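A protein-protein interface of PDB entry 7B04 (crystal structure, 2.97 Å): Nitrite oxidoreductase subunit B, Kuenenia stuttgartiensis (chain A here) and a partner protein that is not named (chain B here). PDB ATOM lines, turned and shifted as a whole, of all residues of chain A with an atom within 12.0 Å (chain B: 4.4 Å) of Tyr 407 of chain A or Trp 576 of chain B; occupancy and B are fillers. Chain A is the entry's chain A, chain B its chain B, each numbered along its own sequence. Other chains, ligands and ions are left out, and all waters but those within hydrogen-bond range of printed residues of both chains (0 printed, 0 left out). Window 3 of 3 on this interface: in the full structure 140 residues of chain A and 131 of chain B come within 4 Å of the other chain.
Printed residues of chain B that touch a printed residue of chain A: Trp 576, Thr 778, Phe 803, Arg 804, Glu 813 and Met 1081. Hydrophobic or aromatic side chains of chain B that line the printed part of chain A: Trp 576, Phe 803 and Met 1081. Among the printed residues, no Asp or Glu carboxylate lies within 4 Å of a Lys or Arg side-chain nitrogen of the other chain.
Among the printed residues, merely in contact across the chains: His 400 of chain A with Arg 804 of chain B (3.6 Å), Ile 401 of chain A with Arg 804 of chain B (3.5 Å), His 406 of chain A with Phe 803 of chain B (3.6 Å), His 406 of chain A with Arg 804 of chain B (3.2 Å), Tyr 407 of chain A with Thr 778 of chain B (3.9 Å), Tyr 407 of chain A with Phe 803 of chain B (3.3 Å), Tyr 407 of chain A with Arg 804 of chain B (3.8 Å), Tyr 407 of chain A with Met 1081 of chain B (3.9 Å), Asn 408 of chain A with Phe 803 of chain B (3.1 Å), Ile 410 of chain A with Phe 803 of chain B (3.5 Å) and Ile 410 of chain A with Met 1081 of chain B (3.9 Å).
Printed residues of chain B within 4 Å of Ile 401 of chain A: Arg 804. Of the printed residues of chain B, His 406 of chain A touches Thr 778, Phe 803 and Arg 804. Of chain B, only Trp 576 (3.2 Å), Thr 778 (3.9 Å), Phe 803 (3.3 Å), Arg 804 (3.8 Å) and Met 1081 (3.9 Å) come within 4 Å of Tyr 407 of chain A. Of the printed residues of chain B, Asn 408 of chain A touches Phe 803 (3.1 Å), Arg 804 (3.1 Å) and Glu 813 (3.3 Å). Of the printed residues of chain B, Ser 409 of chain A touches Glu 813 (3.1 Å). No residue of chain A comes within 4 Å of Ile 417 of chain B. Lys 575 of chain B touches none of the printed residues of chain A. No residue of chain A comes within 4 Å of Ser 577 of chain B. No residue of chain A comes within 4 Å of Gly 578 of chain B. Thr 778 of chain B touches two residues of chain A. No residue of chain A comes within 4 Å of Lys 781 of chain B. Of chain A, only Arg 402, His 406, Tyr 407, Asn 408 and Ile 410 come within 4 Å of Phe 803 of chain B. Of chain A, only Tyr 407 and Ile 410 come within 4 Å of Met 1081 of chain B. The nearest residue of chain B that does not touch Tyr 407 of chain A is Glu 813 of chain B (4.2 Å). The nearest residue of chain A that does not touch Trp 576 of chain B is His 406 of chain A (4.2 Å).
The side-chain amino group (NZ) of Lys 601 of chain B sits at hydrogen-bond distance from the backbone carbonyl oxygen (O) of Trp 576 of chain B, at 3.0 Å. OG of Ser 574 of chain B is in hydrogen-bond range of NE1 of Trp 576 of chain B, 3.2 Å away.
O of Lys 405 of chain A lies close to NE1 of Trp 576 of chain B (3.2 Å). The side-chain carboxylate of Glu 813 of chain B lies within hydrogen-bond range of the backbone NH of Ser 409 of chain A. The side-chain amide oxygen (OD1) of Asn 408 of chain A is in hydrogen-bond range of the backbone NH (N) of Arg 804 of chain B. NH2 of Arg 804 of chain B lies close to O of Pro 403 of chain A (3.0 Å). ND1 of His 406 of chain A sits at hydrogen-bond distance from O of Thr 778 of chain B, 3.3 Å away. N of Asp 404 of chain A sits close to NH2 of Arg 804 of chain B (2.7 Å). The backbone NH (N) of Arg 402 of chain A is in hydrogen-bond range of the backbone carbonyl oxygen (O) of Arg 804 of chain B, 2.8 Å away. The backbone carbonyl oxygen of Phe 803 of chain B lies close to the guanidinium group of Arg 402 of chain A (2.3 Å). The side-chain carboxylate of Glu 813 of chain B sits at hydrogen-bond distance from the backbone NH of Asn 408 of chain A (3.3 Å). The indole nitrogen of Trp 576 of chain B sits at hydrogen-bond distance from the side-chain hydroxyl of Tyr 407 of chain A.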
ATOM      1  N   HIS A 400     -27.867  27.870 -15.505  1.00  0.00           N
ATOM      2  CA  HIS A 400     -26.981  26.823 -15.011  1.00  0.00           C
ATOM      3  C   HIS A 400     -27.762  25.806 -14.189  1.00  0.00           C
ATOM      4  O   HIS A 400     -28.655  26.177 -13.421  1.00  0.00           O
ATOM      5  CB  HIS A 400     -25.865  27.419 -14.155  1.00  0.00           C
ATOM      6  CG  HIS A 400     -25.016  28.412 -14.886  1.00  0.00           C
ATOM      7  ND1 HIS A 400     -24.802  29.691 -14.416  1.00  0.00           N
ATOM      8  CD2 HIS A 400     -24.343  28.319 -16.058  1.00  0.00           C
ATOM      9  CE1 HIS A 400     -24.027  30.341 -15.262  1.00  0.00           C
ATOM     10  NE2 HIS A 400     -23.734  29.532 -16.264  1.00  0.00           N
ATOM     11  N   ILE A 401     -27.367  24.545 -14.291  1.00  0.00           N
ATOM     12  CA  ILE A 401     -27.984  23.455 -13.560  1.00  0.00           C
ATOM     13  C   ILE A 401     -26.884  22.804 -12.747  1.00  0.00           C
ATOM     14  O   ILE A 401     -25.764  22.585 -13.246  1.00  0.00           O
ATOM     15  CB  ILE A 401     -28.628  22.446 -14.518  1.00  0.00           C
ATOM     16  N   ARG A 402     -27.181  22.561 -11.472  1.00  0.00           N
ATOM     17  CA  ARG A 402     -26.245  22.052 -10.494  1.00  0.00           C
ATOM     18  C   ARG A 402     -26.612  20.679  -9.982  1.00  0.00           C
ATOM     19  O   ARG A 402     -27.721  20.177 -10.254  1.00  0.00           O
ATOM     20  CB  ARG A 402     -26.128  23.007  -9.300  1.00  0.00           C
ATOM     21  CG  ARG A 402     -25.575  24.327  -9.702  1.00  0.00           C
ATOM     22  CD  ARG A 402     -24.678  24.833  -8.613  1.00  0.00           C
ATOM     23  NE  ARG A 402     -24.379  26.232  -8.849  1.00  0.00           N
ATOM     24  CZ  ARG A 402     -25.282  27.203  -8.736  1.00  0.00           C
ATOM     25  NH1 ARG A 402     -26.529  26.938  -8.345  1.00  0.00           N
ATOM     26  NH2 ARG A 402     -24.931  28.455  -8.977  1.00  0.00           N
ATOM     27  N   PRO A 403     -25.693  19.985  -9.291  1.00  0.00           N
ATOM     28  CA  PRO A 403     -26.019  18.667  -8.713  1.00  0.00           C
ATOM     29  C   PRO A 403     -27.287  18.716  -7.868  1.00  0.00           C
ATOM     30  O   PRO A 403     -27.628  19.744  -7.279  1.00  0.00           O
ATOM     31  CB  PRO A 403     -24.793  18.347  -7.850  1.00  0.00           C
ATOM     32  CG  PRO A 403     -23.677  19.047  -8.558  1.00  0.00           C
ATOM     33  CD  PRO A 403     -24.227  20.219  -9.328  1.00  0.00           C
ATOM     34  N   ASP A 404     -27.989  17.586  -7.829  1.00  0.00           N
ATOM     35  CA  ASP A 404     -29.265  17.538  -7.133  1.00  0.00           C
ATOM     36  C   ASP A 404     -29.131  17.594  -5.609  1.00  0.00           C
ATOM     37  O   ASP A 404     -30.150  17.737  -4.912  1.00  0.00           O
ATOM     38  CB  ASP A 404     -30.056  16.284  -7.545  1.00  0.00           C
ATOM     39  CG  ASP A 404     -29.191  15.051  -7.587  1.00  0.00           C
ATOM     40  OD1 ASP A 404     -28.049  15.089  -7.092  1.00  0.00           O
ATOM     41  OD2 ASP A 404     -29.674  14.038  -8.119  1.00  0.00           O
ATOM     42  N   LYS A 405     -27.917  17.478  -5.079  1.00  0.00           N
ATOM     43  CA  LYS A 405     -27.671  17.718  -3.661  1.00  0.00           C
ATOM     44  C   LYS A 405     -27.940  19.175  -3.280  1.00  0.00           C
ATOM     45  O   LYS A 405     -28.089  19.478  -2.091  1.00  0.00           O
ATOM     46  CB  LYS A 405     -26.252  17.271  -3.276  1.00  0.00           C
ATOM     47  CG  LYS A 405     -25.129  18.131  -3.781  1.00  0.00           C
ATOM     48  CD  LYS A 405     -23.812  17.522  -3.341  1.00  0.00           C
ATOM     49  CE  LYS A 405     -22.639  18.414  -3.686  1.00  0.00           C
ATOM     50  NZ  LYS A 405     -21.418  18.050  -2.909  1.00  0.00           N
ATOM     51  N   HIS A 406     -27.916  20.088  -4.247  1.00  0.00           N
ATOM     52  CA  HIS A 406     -28.294  21.477  -4.029  1.00  0.00           C
ATOM     53  C   HIS A 406     -29.799  21.631  -4.236  1.00  0.00           C
ATOM     54  O   HIS A 406     -30.426  20.861  -4.974  1.00  0.00           O
ATOM     55  CB  HIS A 406     -27.554  22.404  -4.989  1.00  0.00           C
ATOM     56  CG  HIS A 406     -26.058  22.255  -4.949  1.00  0.00           C
ATOM     57  ND1 HIS A 406     -25.356  21.985  -3.789  1.00  0.00           N
ATOM     58  CD2 HIS A 406     -25.135  22.321  -5.942  1.00  0.00           C
ATOM     59  CE1 HIS A 406     -24.070  21.904  -4.069  1.00  0.00           C
ATOM     60  NE2 HIS A 406     -23.911  22.102  -5.367  1.00  0.00           N
ATOM     61  N   TYR A 407     -30.388  22.617  -3.562  1.00  0.00           N
ATOM     62  CA  TYR A 407     -31.827  22.828  -3.642  1.00  0.00           C
ATOM     63  C   TYR A 407     -32.150  24.286  -3.940  1.00  0.00           C
ATOM     64  O   TYR A 407     -31.399  25.197  -3.579  1.00  0.00           O
ATOM     65  CB  TYR A 407     -32.534  22.407  -2.347  1.00  0.00           C
ATOM     66  CG  TYR A 407     -31.967  21.152  -1.730  1.00  0.00           C
ATOM     67  CD1 TYR A 407     -32.186  19.906  -2.306  1.00  0.00           C
ATOM     68  CD2 TYR A 407     -31.207  21.213  -0.571  1.00  0.00           C
ATOM     69  CE1 TYR A 407     -31.664  18.757  -1.740  1.00  0.00           C
ATOM     70  CE2 TYR A 407     -30.683  20.073   0.001  1.00  0.00           C
ATOM     71  CZ  TYR A 407     -30.914  18.847  -0.586  1.00  0.00           C
ATOM     72  OH  TYR A 407     -30.391  17.710  -0.014  1.00  0.00           O
ATOM     73  N   ASN A 408     -33.285  24.495  -4.607  1.00  0.00           N
ATOM     74  CA  ASN A 408     -33.863  25.818  -4.804  1.00  0.00           C
ATOM     75  C   ASN A 408     -34.956  26.115  -3.790  1.00  0.00           C
ATOM     76  O   ASN A 408     -35.022  27.228  -3.258  1.00  0.00           O
ATOM     77  CB  ASN A 408     -34.454  25.957  -6.212  1.00  0.00           C
ATOM     78  CG  ASN A 408     -33.398  26.099  -7.284  1.00  0.00           C
ATOM     79  OD1 ASN A 408     -32.310  26.611  -7.035  1.00  0.00           O
ATOM     80  ND2 ASN A 408     -33.722  25.663  -8.494  1.00  0.00           N
ATOM     81  N   SER A 409     -35.798  25.123  -3.497  1.00  0.00           N
ATOM     82  CA  SER A 409     -36.925  25.289  -2.582  1.00  0.00           C
ATOM     83  C   SER A 409     -36.413  25.251  -1.142  1.00  0.00           C
ATOM     84  O   SER A 409     -36.605  24.291  -0.392  1.00  0.00           O
ATOM     85  CB  SER A 409     -37.974  24.216  -2.833  1.00  0.00           C
ATOM     86  OG  SER A 409     -38.416  24.241  -4.179  1.00  0.00           O
ATOM     87  N   ILE A 410     -35.743  26.334  -0.763  1.00  0.00           N
ATOM     88  CA  ILE A 410     -35.242  26.494   0.594  1.00  0.00           C
ATOM     89  C   ILE A 410     -35.533  27.910   1.080  1.00  0.00           C
ATOM     90  O   ILE A 410     -35.515  28.864   0.301  1.00  0.00           O
ATOM     91  CB  ILE A 410     -33.736  26.181   0.681  1.00  0.00           C
ATOM     92  CG1 ILE A 410     -32.952  26.993  -0.349  1.00  0.00           C
ATOM     93  CG2 ILE A 410     -33.482  24.690   0.500  1.00  0.00           C
ATOM     94  CD1 ILE A 410     -31.454  26.894  -0.175  1.00  0.00           C
ATOM     95  OXT ILE A 410     -35.795  28.134   2.262  1.00  0.00           O
ATOM     96  N   ILE B 417     -34.860  13.391   1.242  1.00  0.00           N
ATOM     97  CA  ILE B 417     -34.583  14.737   0.754  1.00  0.00           C
ATOM     98  C   ILE B 417     -35.178  15.797   1.675  1.00  0.00           C
ATOM     99  O   ILE B 417     -34.507  16.763   2.038  1.00  0.00           O
ATOM    100  CB  ILE B 417     -35.085  14.916  -0.697  1.00  0.00           C
ATOM    101  CG1 ILE B 417     -34.199  14.135  -1.668  1.00  0.00           C
ATOM    102  CG2 ILE B 417     -35.116  16.389  -1.078  1.00  0.00           C
ATOM    103  CD1 ILE B 417     -34.718  14.119  -3.090  1.00  0.00           C
ATOM    104  N   SER B 574     -28.728  20.120   6.352  1.00  0.00           N
ATOM    105  CA  SER B 574     -29.169  18.839   5.815  1.00  0.00           C
ATOM    106  C   SER B 574     -28.202  17.765   6.306  1.00  0.00           C
ATOM    107  O   SER B 574     -27.201  18.059   6.964  1.00  0.00           O
ATOM    108  CB  SER B 574     -29.274  18.868   4.287  1.00  0.00           C
ATOM    109  OG  SER B 574     -28.003  18.961   3.672  1.00  0.00           O
ATOM    110  N   LYS B 575     -28.514  16.509   5.975  1.00  0.00           N
ATOM    111  CA  LYS B 575     -27.676  15.394   6.412  1.00  0.00           C
ATOM    112  C   LYS B 575     -26.305  15.427   5.745  1.00  0.00           C
ATOM    113  O   LYS B 575     -25.274  15.342   6.423  1.00  0.00           O
ATOM    114  CB  LYS B 575     -28.384  14.069   6.132  1.00  0.00           C
ATOM    115  CG  LYS B 575     -29.837  14.045   6.575  1.00  0.00           C
ATOM    116  N   TRP B 576     -26.271  15.553   4.416  1.00  0.00           N
ATOM    117  CA  TRP B 576     -24.985  15.583   3.730  1.00  0.00           C
ATOM    118  C   TRP B 576     -24.229  16.869   4.035  1.00  0.00           C
ATOM    119  O   TRP B 576     -22.994  16.888   3.984  1.00  0.00           O
ATOM    120  CB  TRP B 576     -25.176  15.419   2.219  1.00  0.00           C
ATOM    121  CG  TRP B 576     -25.782  16.611   1.543  1.00  0.00           C
ATOM    122  CD1 TRP B 576     -27.107  16.830   1.302  1.00  0.00           C
ATOM    123  CD2 TRP B 576     -25.084  17.747   1.014  1.00  0.00           C
ATOM    124  NE1 TRP B 576     -27.278  18.033   0.660  1.00  0.00           N
ATOM    125  CE2 TRP B 576     -26.053  18.616   0.471  1.00  0.00           C
ATOM    126  CE3 TRP B 576     -23.737  18.115   0.949  1.00  0.00           C
ATOM    127  CZ2 TRP B 576     -25.717  19.828  -0.129  1.00  0.00           C
ATOM    128  CZ3 TRP B 576     -23.406  19.320   0.354  1.00  0.00           C
ATOM    129  CH2 TRP B 576     -24.392  20.162  -0.177  1.00  0.00           C
ATOM    130  N   SER B 577     -24.947  17.945   4.357  1.00  0.00           N
ATOM    131  CA  SER B 577     -24.332  19.252   4.562  1.00  0.00           C
ATOM    132  C   SER B 577     -23.873  19.446   6.006  1.00  0.00           C
ATOM    133  O   SER B 577     -22.679  19.616   6.265  1.00  0.00           O
ATOM    134  CB  SER B 577     -25.313  20.361   4.160  1.00  0.00           C
ATOM    135  OG  SER B 577     -26.353  20.487   5.120  1.00  0.00           O
ATOM    136  N   GLY B 578     -24.800  19.407   6.958  1.00  0.00           N
ATOM    137  CA  GLY B 578     -24.451  19.665   8.334  1.00  0.00           C
ATOM    138  C   GLY B 578     -25.438  20.561   9.053  1.00  0.00           C
ATOM    139  O   GLY B 578     -26.601  20.695   8.659  1.00  0.00           O
ATOM    140  N   LYS B 601     -19.534  19.568  11.105  1.00  0.00           N
ATOM    141  CA  LYS B 601     -20.206  18.389  11.632  1.00  0.00           C
ATOM    142  C   LYS B 601     -19.620  17.933  12.961  1.00  0.00           C
ATOM    143  O   LYS B 601     -20.232  17.100  13.637  1.00  0.00           O
ATOM    144  CB  LYS B 601     -20.142  17.247  10.615  1.00  0.00           C
ATOM    145  CG  LYS B 601     -21.004  17.475   9.384  1.00  0.00           C
ATOM    146  CD  LYS B 601     -20.951  16.286   8.440  1.00  0.00           C
ATOM    147  CE  LYS B 601     -21.812  16.522   7.210  1.00  0.00           C
ATOM    148  NZ  LYS B 601     -21.765  15.369   6.269  1.00  0.00           N
ATOM    149  N   THR B 778     -25.928  23.738   2.593  1.00  0.00           N
ATOM    150  CA  THR B 778     -26.160  23.153   1.275  1.00  0.00           C
ATOM    151  C   THR B 778     -25.658  24.066   0.169  1.00  0.00           C
ATOM    152  O   THR B 778     -25.189  23.589  -0.870  1.00  0.00           O
ATOM    153  CB  THR B 778     -27.645  22.857   1.065  1.00  0.00           C
ATOM    154  OG1 THR B 778     -28.373  24.088   0.978  1.00  0.00           O
ATOM    155  CG2 THR B 778     -28.195  22.018   2.206  1.00  0.00           C
ATOM    156  N   LYS B 781     -21.130  24.732   1.467  1.00  0.00           N
ATOM    157  CA  LYS B 781     -20.068  23.785   1.792  1.00  0.00           C
ATOM    158  C   LYS B 781     -19.153  23.616   0.586  1.00  0.00           C
ATOM    159  O   LYS B 781     -19.618  23.404  -0.536  1.00  0.00           O
ATOM    160  CB  LYS B 781     -20.623  22.430   2.231  1.00  0.00           C
ATOM    161  CG  LYS B 781     -19.504  21.493   2.698  1.00  0.00           C
ATOM    162  CD  LYS B 781     -19.974  20.081   2.999  1.00  0.00           C
ATOM    163  CE  LYS B 781     -19.692  19.698   4.442  1.00  0.00           C
ATOM    164  NZ  LYS B 781     -20.527  20.470   5.378  1.00  0.00           N
ATOM    165  N   PHE B 803     -27.300  26.931  -5.273  1.00  0.00           N
ATOM    166  CA  PHE B 803     -28.648  26.408  -5.497  1.00  0.00           C
ATOM    167  C   PHE B 803     -28.580  25.411  -6.656  1.00  0.00           C
ATOM    168  O   PHE B 803     -27.509  25.169  -7.231  1.00  0.00           O
ATOM    169  CB  PHE B 803     -29.649  27.520  -5.816  1.00  0.00           C
ATOM    170  CG  PHE B 803     -29.773  28.556  -4.747  1.00  0.00           C
ATOM    171  CD1 PHE B 803     -30.123  28.223  -3.451  1.00  0.00           C
ATOM    172  CD2 PHE B 803     -29.579  29.885  -5.066  1.00  0.00           C
ATOM    173  CE1 PHE B 803     -30.235  29.202  -2.488  1.00  0.00           C
ATOM    174  CE2 PHE B 803     -29.712  30.865  -4.120  1.00  0.00           C
ATOM    175  CZ  PHE B 803     -30.024  30.526  -2.825  1.00  0.00           C
ATOM    176  N   ARG B 804     -29.735  24.859  -6.988  1.00  0.00           N
ATOM    177  CA  ARG B 804     -29.823  23.963  -8.156  1.00  0.00           C
ATOM    178  C   ARG B 804     -29.694  24.759  -9.447  1.00  0.00           C
ATOM    179  O   ARG B 804     -29.158  24.220 -10.382  1.00  0.00           O
ATOM    180  CB  ARG B 804     -30.973  22.961  -8.090  1.00  0.00           C
ATOM    181  CG  ARG B 804     -30.477  21.540  -8.293  1.00  0.00           C
ATOM    182  CD  ARG B 804     -31.479  20.469  -7.956  1.00  0.00           C
ATOM    183  NE  ARG B 804     -31.761  19.669  -9.132  1.00  0.00           N
ATOM    184  CZ  ARG B 804     -30.858  19.013  -9.816  1.00  0.00           C
ATOM    185  NH1 ARG B 804     -31.226  18.324 -10.874  1.00  0.00           N
ATOM    186  NH2 ARG B 804     -29.598  19.048  -9.441  1.00  0.00           N
ATOM    187  N   GLU B 813     -37.133  21.990  -9.092  1.00  0.00           N
ATOM    188  CA  GLU B 813     -36.933  20.553  -8.949  1.00  0.00           C
ATOM    189  C   GLU B 813     -38.220  19.807  -8.619  1.00  0.00           C
ATOM    190  O   GLU B 813     -38.253  18.579  -8.750  1.00  0.00           O
ATOM    191  CB  GLU B 813     -35.877  20.264  -7.878  1.00  0.00           C
ATOM    192  CG  GLU B 813     -36.275  20.673  -6.476  1.00  0.00           C
ATOM    193  CD  GLU B 813     -35.889  22.102  -6.160  1.00  0.00           C
ATOM    194  OE1 GLU B 813     -35.669  22.886  -7.107  1.00  0.00           O
ATOM    195  OE2 GLU B 813     -35.795  22.440  -4.961  1.00  0.00           O
ATOM    196  N   MET B1081     -33.527  21.160   6.193  1.00  0.00           N
ATOM    197  CA  MET B1081     -34.367  20.357   5.313  1.00  0.00           C
ATOM    198  C   MET B1081     -35.201  19.405   6.158  1.00  0.00           C
ATOM    199  O   MET B1081     -34.979  18.189   6.150  1.00  0.00           O
ATOM    200  CB  MET B1081     -33.521  19.580   4.300  1.00  0.00           C
ATOM    201  CG  MET B1081     -32.877  20.441   3.226  1.00  0.00           C
ATOM    202  SD  MET B1081     -34.086  21.273   2.177  1.00  0.00           S
ATOM    203  CE  MET B1081     -34.748  19.894   1.246  1.00  0.00           C
